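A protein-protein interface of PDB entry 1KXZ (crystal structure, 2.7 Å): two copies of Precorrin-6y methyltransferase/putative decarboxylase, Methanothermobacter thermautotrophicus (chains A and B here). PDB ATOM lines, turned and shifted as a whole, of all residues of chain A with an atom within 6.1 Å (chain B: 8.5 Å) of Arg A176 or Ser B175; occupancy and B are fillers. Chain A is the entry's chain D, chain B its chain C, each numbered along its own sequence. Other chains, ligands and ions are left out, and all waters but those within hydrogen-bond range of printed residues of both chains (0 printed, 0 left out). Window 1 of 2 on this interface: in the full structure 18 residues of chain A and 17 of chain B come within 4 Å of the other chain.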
ATOM      1  N   ALA A  18     -22.874 -28.241  -9.022  1.00  0.00           N
ATOM      2  CA  ALA A  18     -23.072 -29.673  -9.137  1.00  0.00           C
ATOM      3  C   ALA A  18     -22.058 -30.426  -8.303  1.00  0.00           C
ATOM      4  O   ALA A  18     -20.879 -30.129  -8.345  1.00  0.00           O
ATOM      5  CB  ALA A  18     -22.968 -30.090 -10.592  1.00  0.00           C
ATOM      6  N   GLU A  20     -20.632 -33.020  -8.807  1.00  0.00           N
ATOM      7  CA  GLU A  20     -19.573 -33.538  -9.663  1.00  0.00           C
ATOM      8  C   GLU A  20     -18.517 -32.500  -9.853  1.00  0.00           C
ATOM      9  O   GLU A  20     -17.344 -32.826  -9.930  1.00  0.00           O
ATOM     10  CB  GLU A  20     -20.109 -34.009 -11.001  1.00  0.00           C
ATOM     11  CG  GLU A  20     -21.070 -35.199 -10.906  1.00  0.00           C
ATOM     12  CD  GLU A  20     -22.542 -34.874 -10.487  1.00  0.00           C
ATOM     13  OE1 GLU A  20     -22.963 -33.697 -10.443  1.00  0.00           O
ATOM     14  OE2 GLU A  20     -23.310 -35.832 -10.224  1.00  0.00           O
ATOM     15  N   LEU A 159     -16.689 -29.857 -17.881  1.00  0.00           N
ATOM     16  CA  LEU A 159     -17.450 -30.982 -17.390  1.00  0.00           C
ATOM     17  C   LEU A 159     -18.871 -30.949 -17.895  1.00  0.00           C
ATOM     18  O   LEU A 159     -19.581 -29.968 -17.700  1.00  0.00           O
ATOM     19  CB  LEU A 159     -17.473 -30.994 -15.861  1.00  0.00           C
ATOM     20  CG  LEU A 159     -16.285 -31.612 -15.145  1.00  0.00           C
ATOM     21  CD1 LEU A 159     -16.575 -31.697 -13.668  1.00  0.00           C
ATOM     22  CD2 LEU A 159     -16.083 -33.022 -15.689  1.00  0.00           C
ATOM     23  N   ASN A 160     -19.285 -32.008 -18.571  1.00  0.00           N
ATOM     24  CA  ASN A 160     -20.660 -32.096 -19.024  1.00  0.00           C
ATOM     25  C   ASN A 160     -21.232 -33.277 -18.270  1.00  0.00           C
ATOM     26  O   ASN A 160     -20.906 -34.422 -18.567  1.00  0.00           O
ATOM     27  CB  ASN A 160     -20.736 -32.314 -20.523  1.00  0.00           C
ATOM     28  CG  ASN A 160     -20.565 -31.032 -21.298  1.00  0.00           C
ATOM     29  OD1 ASN A 160     -21.543 -30.440 -21.756  1.00  0.00           O
ATOM     30  ND2 ASN A 160     -19.324 -30.582 -21.439  1.00  0.00           N
ATOM     31  N   ILE A 161     -22.019 -32.990 -17.241  1.00  0.00           N
ATOM     32  CA  ILE A 161     -22.599 -34.033 -16.427  1.00  0.00           C
ATOM     33  C   ILE A 161     -24.048 -34.234 -16.777  1.00  0.00           C
ATOM     34  O   ILE A 161     -24.717 -33.270 -17.144  1.00  0.00           O
ATOM     35  CB  ILE A 161     -22.538 -33.645 -14.952  1.00  0.00           C
ATOM     36  CG1 ILE A 161     -21.147 -33.147 -14.621  1.00  0.00           C
ATOM     37  CG2 ILE A 161     -22.872 -34.845 -14.064  1.00  0.00           C
ATOM     38  CD1 ILE A 161     -21.176 -31.877 -13.864  1.00  0.00           C
ATOM     39  N   ALA A 162     -24.515 -35.479 -16.655  1.00  0.00           N
ATOM     40  CA  ALA A 162     -25.894 -35.852 -16.901  1.00  0.00           C
ATOM     41  C   ALA A 162     -26.224 -36.811 -15.768  1.00  0.00           C
ATOM     42  O   ALA A 162     -25.405 -37.612 -15.385  1.00  0.00           O
ATOM     43  CB  ALA A 162     -26.020 -36.539 -18.253  1.00  0.00           C
ATOM     44  N   ARG A 163     -27.380 -36.651 -15.150  1.00  0.00           N
ATOM     45  CA  ARG A 163     -27.792 -37.550 -14.085  1.00  0.00           C
ATOM     46  C   ARG A 163     -29.079 -38.158 -14.531  1.00  0.00           C
ATOM     47  O   ARG A 163     -29.832 -37.517 -15.239  1.00  0.00           O
ATOM     48  CB  ARG A 163     -28.028 -36.783 -12.801  1.00  0.00           C
ATOM     49  CG  ARG A 163     -26.851 -35.969 -12.368  1.00  0.00           C
ATOM     50  CD  ARG A 163     -27.028 -35.571 -10.948  1.00  0.00           C
ATOM     51  NE  ARG A 163     -26.045 -34.569 -10.571  1.00  0.00           N
ATOM     52  CZ  ARG A 163     -26.363 -33.357 -10.117  1.00  0.00           C
ATOM     53  NH1 ARG A 163     -27.642 -32.998  -9.994  1.00  0.00           N
ATOM     54  NH2 ARG A 163     -25.409 -32.509  -9.747  1.00  0.00           N
ATOM     55  N   ARG A 165     -32.857 -39.400 -14.252  1.00  0.00           N
ATOM     56  CA  ARG A 165     -34.018 -39.064 -13.457  1.00  0.00           C
ATOM     57  C   ARG A 165     -34.949 -40.219 -13.713  1.00  0.00           C
ATOM     58  O   ARG A 165     -35.216 -40.544 -14.887  1.00  0.00           O
ATOM     59  CB  ARG A 165     -34.638 -37.781 -13.946  1.00  0.00           C
ATOM     60  CG  ARG A 165     -35.940 -37.453 -13.187  1.00  0.00           C
ATOM     61  CD  ARG A 165     -36.713 -36.270 -13.813  1.00  0.00           C
ATOM     62  NE  ARG A 165     -35.972 -35.015 -13.701  1.00  0.00           N
ATOM     63  CZ  ARG A 165     -35.965 -34.057 -14.626  1.00  0.00           C
ATOM     64  NH1 ARG A 165     -36.664 -34.200 -15.757  1.00  0.00           N
ATOM     65  NH2 ARG A 165     -35.238 -32.959 -14.423  1.00  0.00           N
ATOM     66  N   VAL A 174     -30.429 -36.351 -17.653  1.00  0.00           N
ATOM     67  CA  VAL A 174     -30.688 -34.929 -17.607  1.00  0.00           C
ATOM     68  C   VAL A 174     -29.409 -34.171 -17.406  1.00  0.00           C
ATOM     69  O   VAL A 174     -28.734 -34.286 -16.384  1.00  0.00           O
ATOM     70  CB  VAL A 174     -31.620 -34.534 -16.462  1.00  0.00           C
ATOM     71  CG1 VAL A 174     -31.796 -33.036 -16.450  1.00  0.00           C
ATOM     72  CG2 VAL A 174     -32.964 -35.239 -16.588  1.00  0.00           C
ATOM     73  N   SER A 175     -29.152 -33.282 -18.339  1.00  0.00           N
ATOM     74  CA  SER A 175     -27.928 -32.506 -18.323  1.00  0.00           C
ATOM     75  C   SER A 175     -27.893 -31.299 -17.466  1.00  0.00           C
ATOM     76  O   SER A 175     -28.897 -30.636 -17.260  1.00  0.00           O
ATOM     77  CB  SER A 175     -27.563 -32.054 -19.724  1.00  0.00           C
ATOM     78  OG  SER A 175     -27.155 -33.152 -20.524  1.00  0.00           O
ATOM     79  N   ARG A 176     -26.717 -31.054 -16.917  1.00  0.00           N
ATOM     80  CA  ARG A 176     -26.442 -29.870 -16.114  1.00  0.00           C
ATOM     81  C   ARG A 176     -25.793 -29.016 -17.197  1.00  0.00           C
ATOM     82  O   ARG A 176     -25.292 -29.548 -18.186  1.00  0.00           O
ATOM     83  CB  ARG A 176     -25.356 -30.132 -15.048  1.00  0.00           C
ATOM     84  CG  ARG A 176     -25.680 -31.073 -13.926  1.00  0.00           C
ATOM     85  CD  ARG A 176     -26.919 -30.635 -13.203  1.00  0.00           C
ATOM     86  NE  ARG A 176     -28.026 -31.516 -13.570  1.00  0.00           N
ATOM     87  CZ  ARG A 176     -29.241 -31.449 -13.045  1.00  0.00           C
ATOM     88  NH1 ARG A 176     -29.517 -30.522 -12.131  1.00  0.00           N
ATOM     89  NH2 ARG A 176     -30.159 -32.349 -13.378  1.00  0.00           N
ATOM     90  N   ASN A 177     -25.776 -27.704 -17.038  1.00  0.00           N
ATOM     91  CA  ASN A 177     -25.111 -26.896 -18.058  1.00  0.00           C
ATOM     92  C   ASN A 177     -23.626 -27.136 -17.912  1.00  0.00           C
ATOM     93  O   ASN A 177     -23.140 -27.412 -16.804  1.00  0.00           O
ATOM     94  CB  ASN A 177     -25.378 -25.420 -17.885  1.00  0.00           C
ATOM     95  CG  ASN A 177     -26.762 -25.073 -18.194  1.00  0.00           C
ATOM     96  OD1 ASN A 177     -27.451 -25.805 -18.913  1.00  0.00           O
ATOM     97  ND2 ASN A 177     -27.232 -23.980 -17.629  1.00  0.00           N
ATOM     98  N   PRO A 178     -22.873 -27.000 -19.013  1.00  0.00           N
ATOM     99  CA  PRO A 178     -21.430 -27.209 -19.027  1.00  0.00           C
ATOM    100  C   PRO A 178     -20.788 -26.293 -18.052  1.00  0.00           C
ATOM    101  O   PRO A 178     -21.202 -25.152 -17.917  1.00  0.00           O
ATOM    102  CB  PRO A 178     -21.042 -26.768 -20.419  1.00  0.00           C
ATOM    103  CG  PRO A 178     -22.263 -26.994 -21.212  1.00  0.00           C
ATOM    104  CD  PRO A 178     -23.310 -26.475 -20.309  1.00  0.00           C
ATOM    105  N   VAL A 179     -19.761 -26.776 -17.378  1.00  0.00           N
ATOM    106  CA  VAL A 179     -19.038 -25.975 -16.405  1.00  0.00           C
ATOM    107  C   VAL A 179     -17.574 -26.221 -16.680  1.00  0.00           C
ATOM    108  O   VAL A 179     -17.152 -27.354 -16.816  1.00  0.00           O
ATOM    109  CB  VAL A 179     -19.323 -26.396 -14.939  1.00  0.00           C
ATOM    110  CG1 VAL A 179     -18.519 -25.519 -13.985  1.00  0.00           C
ATOM    111  CG2 VAL A 179     -20.811 -26.263 -14.634  1.00  0.00           C
ATOM    112  N   LEU B 159     -25.187 -37.134 -28.812  1.00  0.00           N
ATOM    113  CA  LEU B 159     -24.960 -35.718 -29.027  1.00  0.00           C
ATOM    114  C   LEU B 159     -25.161 -34.902 -27.764  1.00  0.00           C
ATOM    115  O   LEU B 159     -26.181 -35.012 -27.108  1.00  0.00           O
ATOM    116  CB  LEU B 159     -25.892 -35.182 -30.097  1.00  0.00           C
ATOM    117  CG  LEU B 159     -25.479 -35.399 -31.537  1.00  0.00           C
ATOM    118  CD1 LEU B 159     -26.469 -34.670 -32.433  1.00  0.00           C
ATOM    119  CD2 LEU B 159     -24.055 -34.842 -31.741  1.00  0.00           C
ATOM    120  N   ASN B 160     -24.156 -34.135 -27.387  1.00  0.00           N
ATOM    121  CA  ASN B 160     -24.276 -33.253 -26.246  1.00  0.00           C
ATOM    122  C   ASN B 160     -24.119 -31.842 -26.818  1.00  0.00           C
ATOM    123  O   ASN B 160     -23.013 -31.414 -27.190  1.00  0.00           O
ATOM    124  CB  ASN B 160     -23.205 -33.548 -25.210  1.00  0.00           C
ATOM    125  CG  ASN B 160     -23.548 -34.730 -24.361  1.00  0.00           C
ATOM    126  OD1 ASN B 160     -24.020 -34.577 -23.236  1.00  0.00           O
ATOM    127  ND2 ASN B 160     -23.338 -35.921 -24.893  1.00  0.00           N
ATOM    128  N   ILE B 161     -25.244 -31.158 -26.975  1.00  0.00           N
ATOM    129  CA  ILE B 161     -25.239 -29.814 -27.518  1.00  0.00           C
ATOM    130  C   ILE B 161     -25.380 -28.755 -26.456  1.00  0.00           C
ATOM    131  O   ILE B 161     -26.069 -28.971 -25.472  1.00  0.00           O
ATOM    132  CB  ILE B 161     -26.371 -29.617 -28.480  1.00  0.00           C
ATOM    133  CG1 ILE B 161     -26.397 -30.790 -29.437  1.00  0.00           C
ATOM    134  CG2 ILE B 161     -26.208 -28.302 -29.244  1.00  0.00           C
ATOM    135  CD1 ILE B 161     -27.810 -31.352 -29.578  1.00  0.00           C
ATOM    136  N   ALA B 162     -24.725 -27.616 -26.667  1.00  0.00           N
ATOM    137  CA  ALA B 162     -24.772 -26.501 -25.748  1.00  0.00           C
ATOM    138  C   ALA B 162     -24.855 -25.302 -26.661  1.00  0.00           C
ATOM    139  O   ALA B 162     -24.157 -25.237 -27.666  1.00  0.00           O
ATOM    140  CB  ALA B 162     -23.485 -26.441 -24.895  1.00  0.00           C
ATOM    141  N   ARG B 163     -25.782 -24.403 -26.373  1.00  0.00           N
ATOM    142  CA  ARG B 163     -25.929 -23.181 -27.152  1.00  0.00           C
ATOM    143  C   ARG B 163     -25.660 -22.022 -26.236  1.00  0.00           C
ATOM    144  O   ARG B 163     -25.890 -22.110 -25.045  1.00  0.00           O
ATOM    145  CB  ARG B 163     -27.335 -23.078 -27.681  1.00  0.00           C
ATOM    146  CG  ARG B 163     -27.778 -24.307 -28.422  1.00  0.00           C
ATOM    147  CD  ARG B 163     -28.996 -23.982 -29.200  1.00  0.00           C
ATOM    148  NE  ARG B 163     -29.598 -25.179 -29.754  1.00  0.00           N
ATOM    149  CZ  ARG B 163     -30.842 -25.570 -29.491  1.00  0.00           C
ATOM    150  NH1 ARG B 163     -31.622 -24.857 -28.674  1.00  0.00           N
ATOM    151  NH2 ARG B 163     -31.322 -26.672 -30.060  1.00  0.00           N
ATOM    152  N   GLY B 164     -25.132 -20.945 -26.755  1.00  0.00           N
ATOM    153  CA  GLY B 164     -24.850 -19.850 -25.860  1.00  0.00           C
ATOM    154  C   GLY B 164     -26.084 -19.013 -25.697  1.00  0.00           C
ATOM    155  O   GLY B 164     -26.860 -18.884 -26.615  1.00  0.00           O
ATOM    156  N   ARG B 165     -26.289 -18.473 -24.512  1.00  0.00           N
ATOM    157  CA  ARG B 165     -27.425 -17.617 -24.245  1.00  0.00           C
ATOM    158  C   ARG B 165     -26.751 -16.324 -23.845  1.00  0.00           C
ATOM    159  O   ARG B 165     -25.902 -16.306 -22.953  1.00  0.00           O
ATOM    160  CB  ARG B 165     -28.237 -18.157 -23.077  1.00  0.00           C
ATOM    161  CG  ARG B 165     -29.372 -17.246 -22.673  1.00  0.00           C
ATOM    162  CD  ARG B 165     -30.088 -17.652 -21.359  1.00  0.00           C
ATOM    163  NE  ARG B 165     -30.779 -18.931 -21.486  1.00  0.00           N
ATOM    164  CZ  ARG B 165     -30.878 -19.841 -20.521  1.00  0.00           C
ATOM    165  NH1 ARG B 165     -30.325 -19.627 -19.324  1.00  0.00           N
ATOM    166  NH2 ARG B 165     -31.525 -20.983 -20.764  1.00  0.00           N
ATOM    167  N   MET B 172     -23.345 -17.444 -22.004  1.00  0.00           N
ATOM    168  CA  MET B 172     -23.308 -18.600 -21.150  1.00  0.00           C
ATOM    169  C   MET B 172     -23.688 -19.843 -21.928  1.00  0.00           C
ATOM    170  O   MET B 172     -24.662 -19.825 -22.654  1.00  0.00           O
ATOM    171  CB  MET B 172     -24.321 -18.394 -20.064  1.00  0.00           C
ATOM    172  CG  MET B 172     -24.497 -19.591 -19.189  1.00  0.00           C
ATOM    173  SD  MET B 172     -26.169 -19.396 -18.217  1.00  0.00           S
ATOM    174  CE  MET B 172     -27.210 -18.581 -19.553  1.00  0.00           C
ATOM    175  N   MET B 173     -22.972 -20.947 -21.750  1.00  0.00           N
ATOM    176  CA  MET B 173     -23.303 -22.170 -22.508  1.00  0.00           C
ATOM    177  C   MET B 173     -24.423 -22.927 -21.836  1.00  0.00           C
ATOM    178  O   MET B 173     -24.350 -23.253 -20.644  1.00  0.00           O
ATOM    179  CB  MET B 173     -22.079 -23.082 -22.669  1.00  0.00           C
ATOM    180  CG  MET B 173     -20.941 -22.451 -23.482  1.00  0.00           C
ATOM    181  SD  MET B 173     -21.607 -21.696 -25.227  1.00  0.00           S
ATOM    182  CE  MET B 173     -21.880 -23.343 -26.160  1.00  0.00           C
ATOM    183  N   VAL B 174     -25.475 -23.204 -22.588  1.00  0.00           N
ATOM    184  CA  VAL B 174     -26.615 -23.904 -22.032  1.00  0.00           C
ATOM    185  C   VAL B 174     -26.818 -25.229 -22.712  1.00  0.00           C
ATOM    186  O   VAL B 174     -27.142 -25.289 -23.889  1.00  0.00           O
ATOM    187  CB  VAL B 174     -27.913 -23.118 -22.162  1.00  0.00           C
ATOM    188  CG1 VAL B 174     -29.030 -23.928 -21.532  1.00  0.00           C
ATOM    189  CG2 VAL B 174     -27.814 -21.798 -21.444  1.00  0.00           C
ATOM    190  N   SER B 175     -26.742 -26.284 -21.919  1.00  0.00           N
ATOM    191  CA  SER B 175     -26.868 -27.644 -22.398  1.00  0.00           C
ATOM    192  C   SER B 175     -28.260 -28.132 -22.630  1.00  0.00           C
ATOM    193  O   SER B 175     -29.194 -27.757 -21.936  1.00  0.00           O
ATOM    194  CB  SER B 175     -26.186 -28.608 -21.429  1.00  0.00           C
ATOM    195  OG  SER B 175     -24.781 -28.499 -21.519  1.00  0.00           O
ATOM    196  N   ARG B 176     -28.383 -28.948 -23.669  1.00  0.00           N
ATOM    197  CA  ARG B 176     -29.614 -29.631 -24.010  1.00  0.00           C
ATOM    198  C   ARG B 176     -29.300 -30.989 -23.398  1.00  0.00           C
ATOM    199  O   ARG B 176     -28.122 -31.372 -23.283  1.00  0.00           O
ATOM    200  CB  ARG B 176     -29.737 -29.884 -25.509  1.00  0.00           C
ATOM    201  CG  ARG B 176     -29.872 -28.711 -26.399  1.00  0.00           C
ATOM    202  CD  ARG B 176     -31.048 -27.894 -25.991  1.00  0.00           C
ATOM    203  NE  ARG B 176     -30.592 -26.689 -25.305  1.00  0.00           N
ATOM    204  CZ  ARG B 176     -31.389 -25.705 -24.898  1.00  0.00           C
ATOM    205  NH1 ARG B 176     -32.696 -25.797 -25.098  1.00  0.00           N
ATOM    206  NH2 ARG B 176     -30.874 -24.598 -24.369  1.00  0.00           N
ATOM    207  N   ASN B 177     -30.313 -31.761 -23.058  1.00  0.00           N
ATOM    208  CA  ASN B 177     -30.012 -33.066 -22.511  1.00  0.00           C
ATOM    209  C   ASN B 177     -29.390 -33.926 -23.603  1.00  0.00           C
ATOM    210  O   ASN B 177     -29.653 -33.733 -24.790  1.00  0.00           O
ATOM    211  CB  ASN B 177     -31.267 -33.719 -21.973  1.00  0.00           C
ATOM    212  CG  ASN B 177     -31.812 -32.996 -20.813  1.00  0.00           C
ATOM    213  OD1 ASN B 177     -31.089 -32.283 -20.113  1.00  0.00           O
ATOM    214  ND2 ASN B 177     -33.091 -33.173 -20.566  1.00  0.00           N
ATOM    215  N   PRO B 178     -28.574 -34.914 -23.216  1.00  0.00           N
ATOM    216  CA  PRO B 178     -27.933 -35.796 -24.181  1.00  0.00           C
ATOM    217  C   PRO B 178     -28.976 -36.492 -24.991  1.00  0.00           C
ATOM    218  O   PRO B 178     -30.013 -36.875 -24.451  1.00  0.00           O
ATOM    219  CB  PRO B 178     -27.251 -36.828 -23.280  1.00  0.00           C
ATOM    220  CG  PRO B 178     -27.007 -36.090 -22.027  1.00  0.00           C
ATOM    221  CD  PRO B 178     -28.296 -35.379 -21.852  1.00  0.00           C
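OG of Ser A175 sits at hydrogen-bond distance from O of Arg B176, 3.4 Å away. OD1 of Asn B177 lies within hydrogen-bond range of N of Ser A175 (2.8 Å). The backbone NH (N) of Ser B175 is in hydrogen-bond range of the side-chain amide oxygen (OD1) of Asn A177 (3.1 Å). N of Pro A178 lies close to OG of Ser B175 (3.5 Å).
Printed residues of chain B within 4 Å of Val A174: Asn B177. Of chain B, only Arg B176 (3.4 Å), Asn B177 (2.8 Å) and Pro B178 (2.8 Å) come within 4 Å of Ser A175. Arg A176 touches just one residue of chain B: Ser B175 (3.5 Å). Of the printed residues of chain A, Ala B162 touches Pro A178. Arg B165 touches none of the printed residues of chain A. Of chain A, only Asn A160 (3.8 Å), Arg A176 (3.5 Å), Asn A177 (3.1 Å) and Pro A178 (2.8 Å) come within 4 Å of Ser B175. The nearest residue of chain B that does not touch Arg A176 is Asn B177 (5.6 Å).
Among the printed residues, merely in contact across the chains: Ser A175 with Pro B178, Pro A178 with Met B173, Arg A176 with Ser B175, Asn A177 with Val B174, Asn A177 with Met B173, Val A174 with Asn B177, Asn A160 with Ser B175, Pro A178 with Ala B162 and Ala A162 with Pro B178.
Printed residues of chain A that touch a printed residue of chain B: Asn A160, Ala A162, Val A174, Ser A175, Arg A176, Asn A177 and Pro A178. Hydrophobic or aromatic side chains of chain A within 4 Å of the printed part of chain B: Ala A162, Val A174 and Pro A178. Of the 14 printed residues of chain B, 7 touch a printed residue of chain A. Hydrophobic or aromatic side chains of chain B within 4 Å of the printed part of chain A: Ala B162, Val B174 and Pro B178. Among the printed residues, 13 pairs touch across the chains. Among the printed residues, no Asp or Glu carboxylate lies within 4 Å of a Lys or Arg side-chain nitrogen of the other chain.
N of Val B174 sits at hydrogen-bond distance from O of Arg B163 (2.7 Å). The backbone carbonyl oxygen (O) of Arg A163 sits at hydrogen-bond distance from the backbone NH (N) of Val A174 (2.7 Å). The backbone NH (N) of Arg B176 lies within hydrogen-bond range of the backbone carbonyl oxygen (O) of Ile B161. The backbone NH (N) of Arg A176 sits at hydrogen-bond distance from the backbone carbonyl oxygen (O) of Ile A161, at 3.0 Å.
Asn A160 touches Ser B175, but with the chains exchanged Ser A175 does not touch Asn B160 (4.4 Å). Val A174 touches Asn B177, and with the chains exchanged Asn A177 touches Val B174. Ser A175 touches Arg B176, and with the chains exchanged Arg A176 touches Ser B175. Ser A175 touches Asn B177, and with the chains exchanged Asn A177 touches Ser B175. Positions printed for both chains: 159, 160, 161, 162, 163, 165, 174, 175, 176, 177 and 178.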
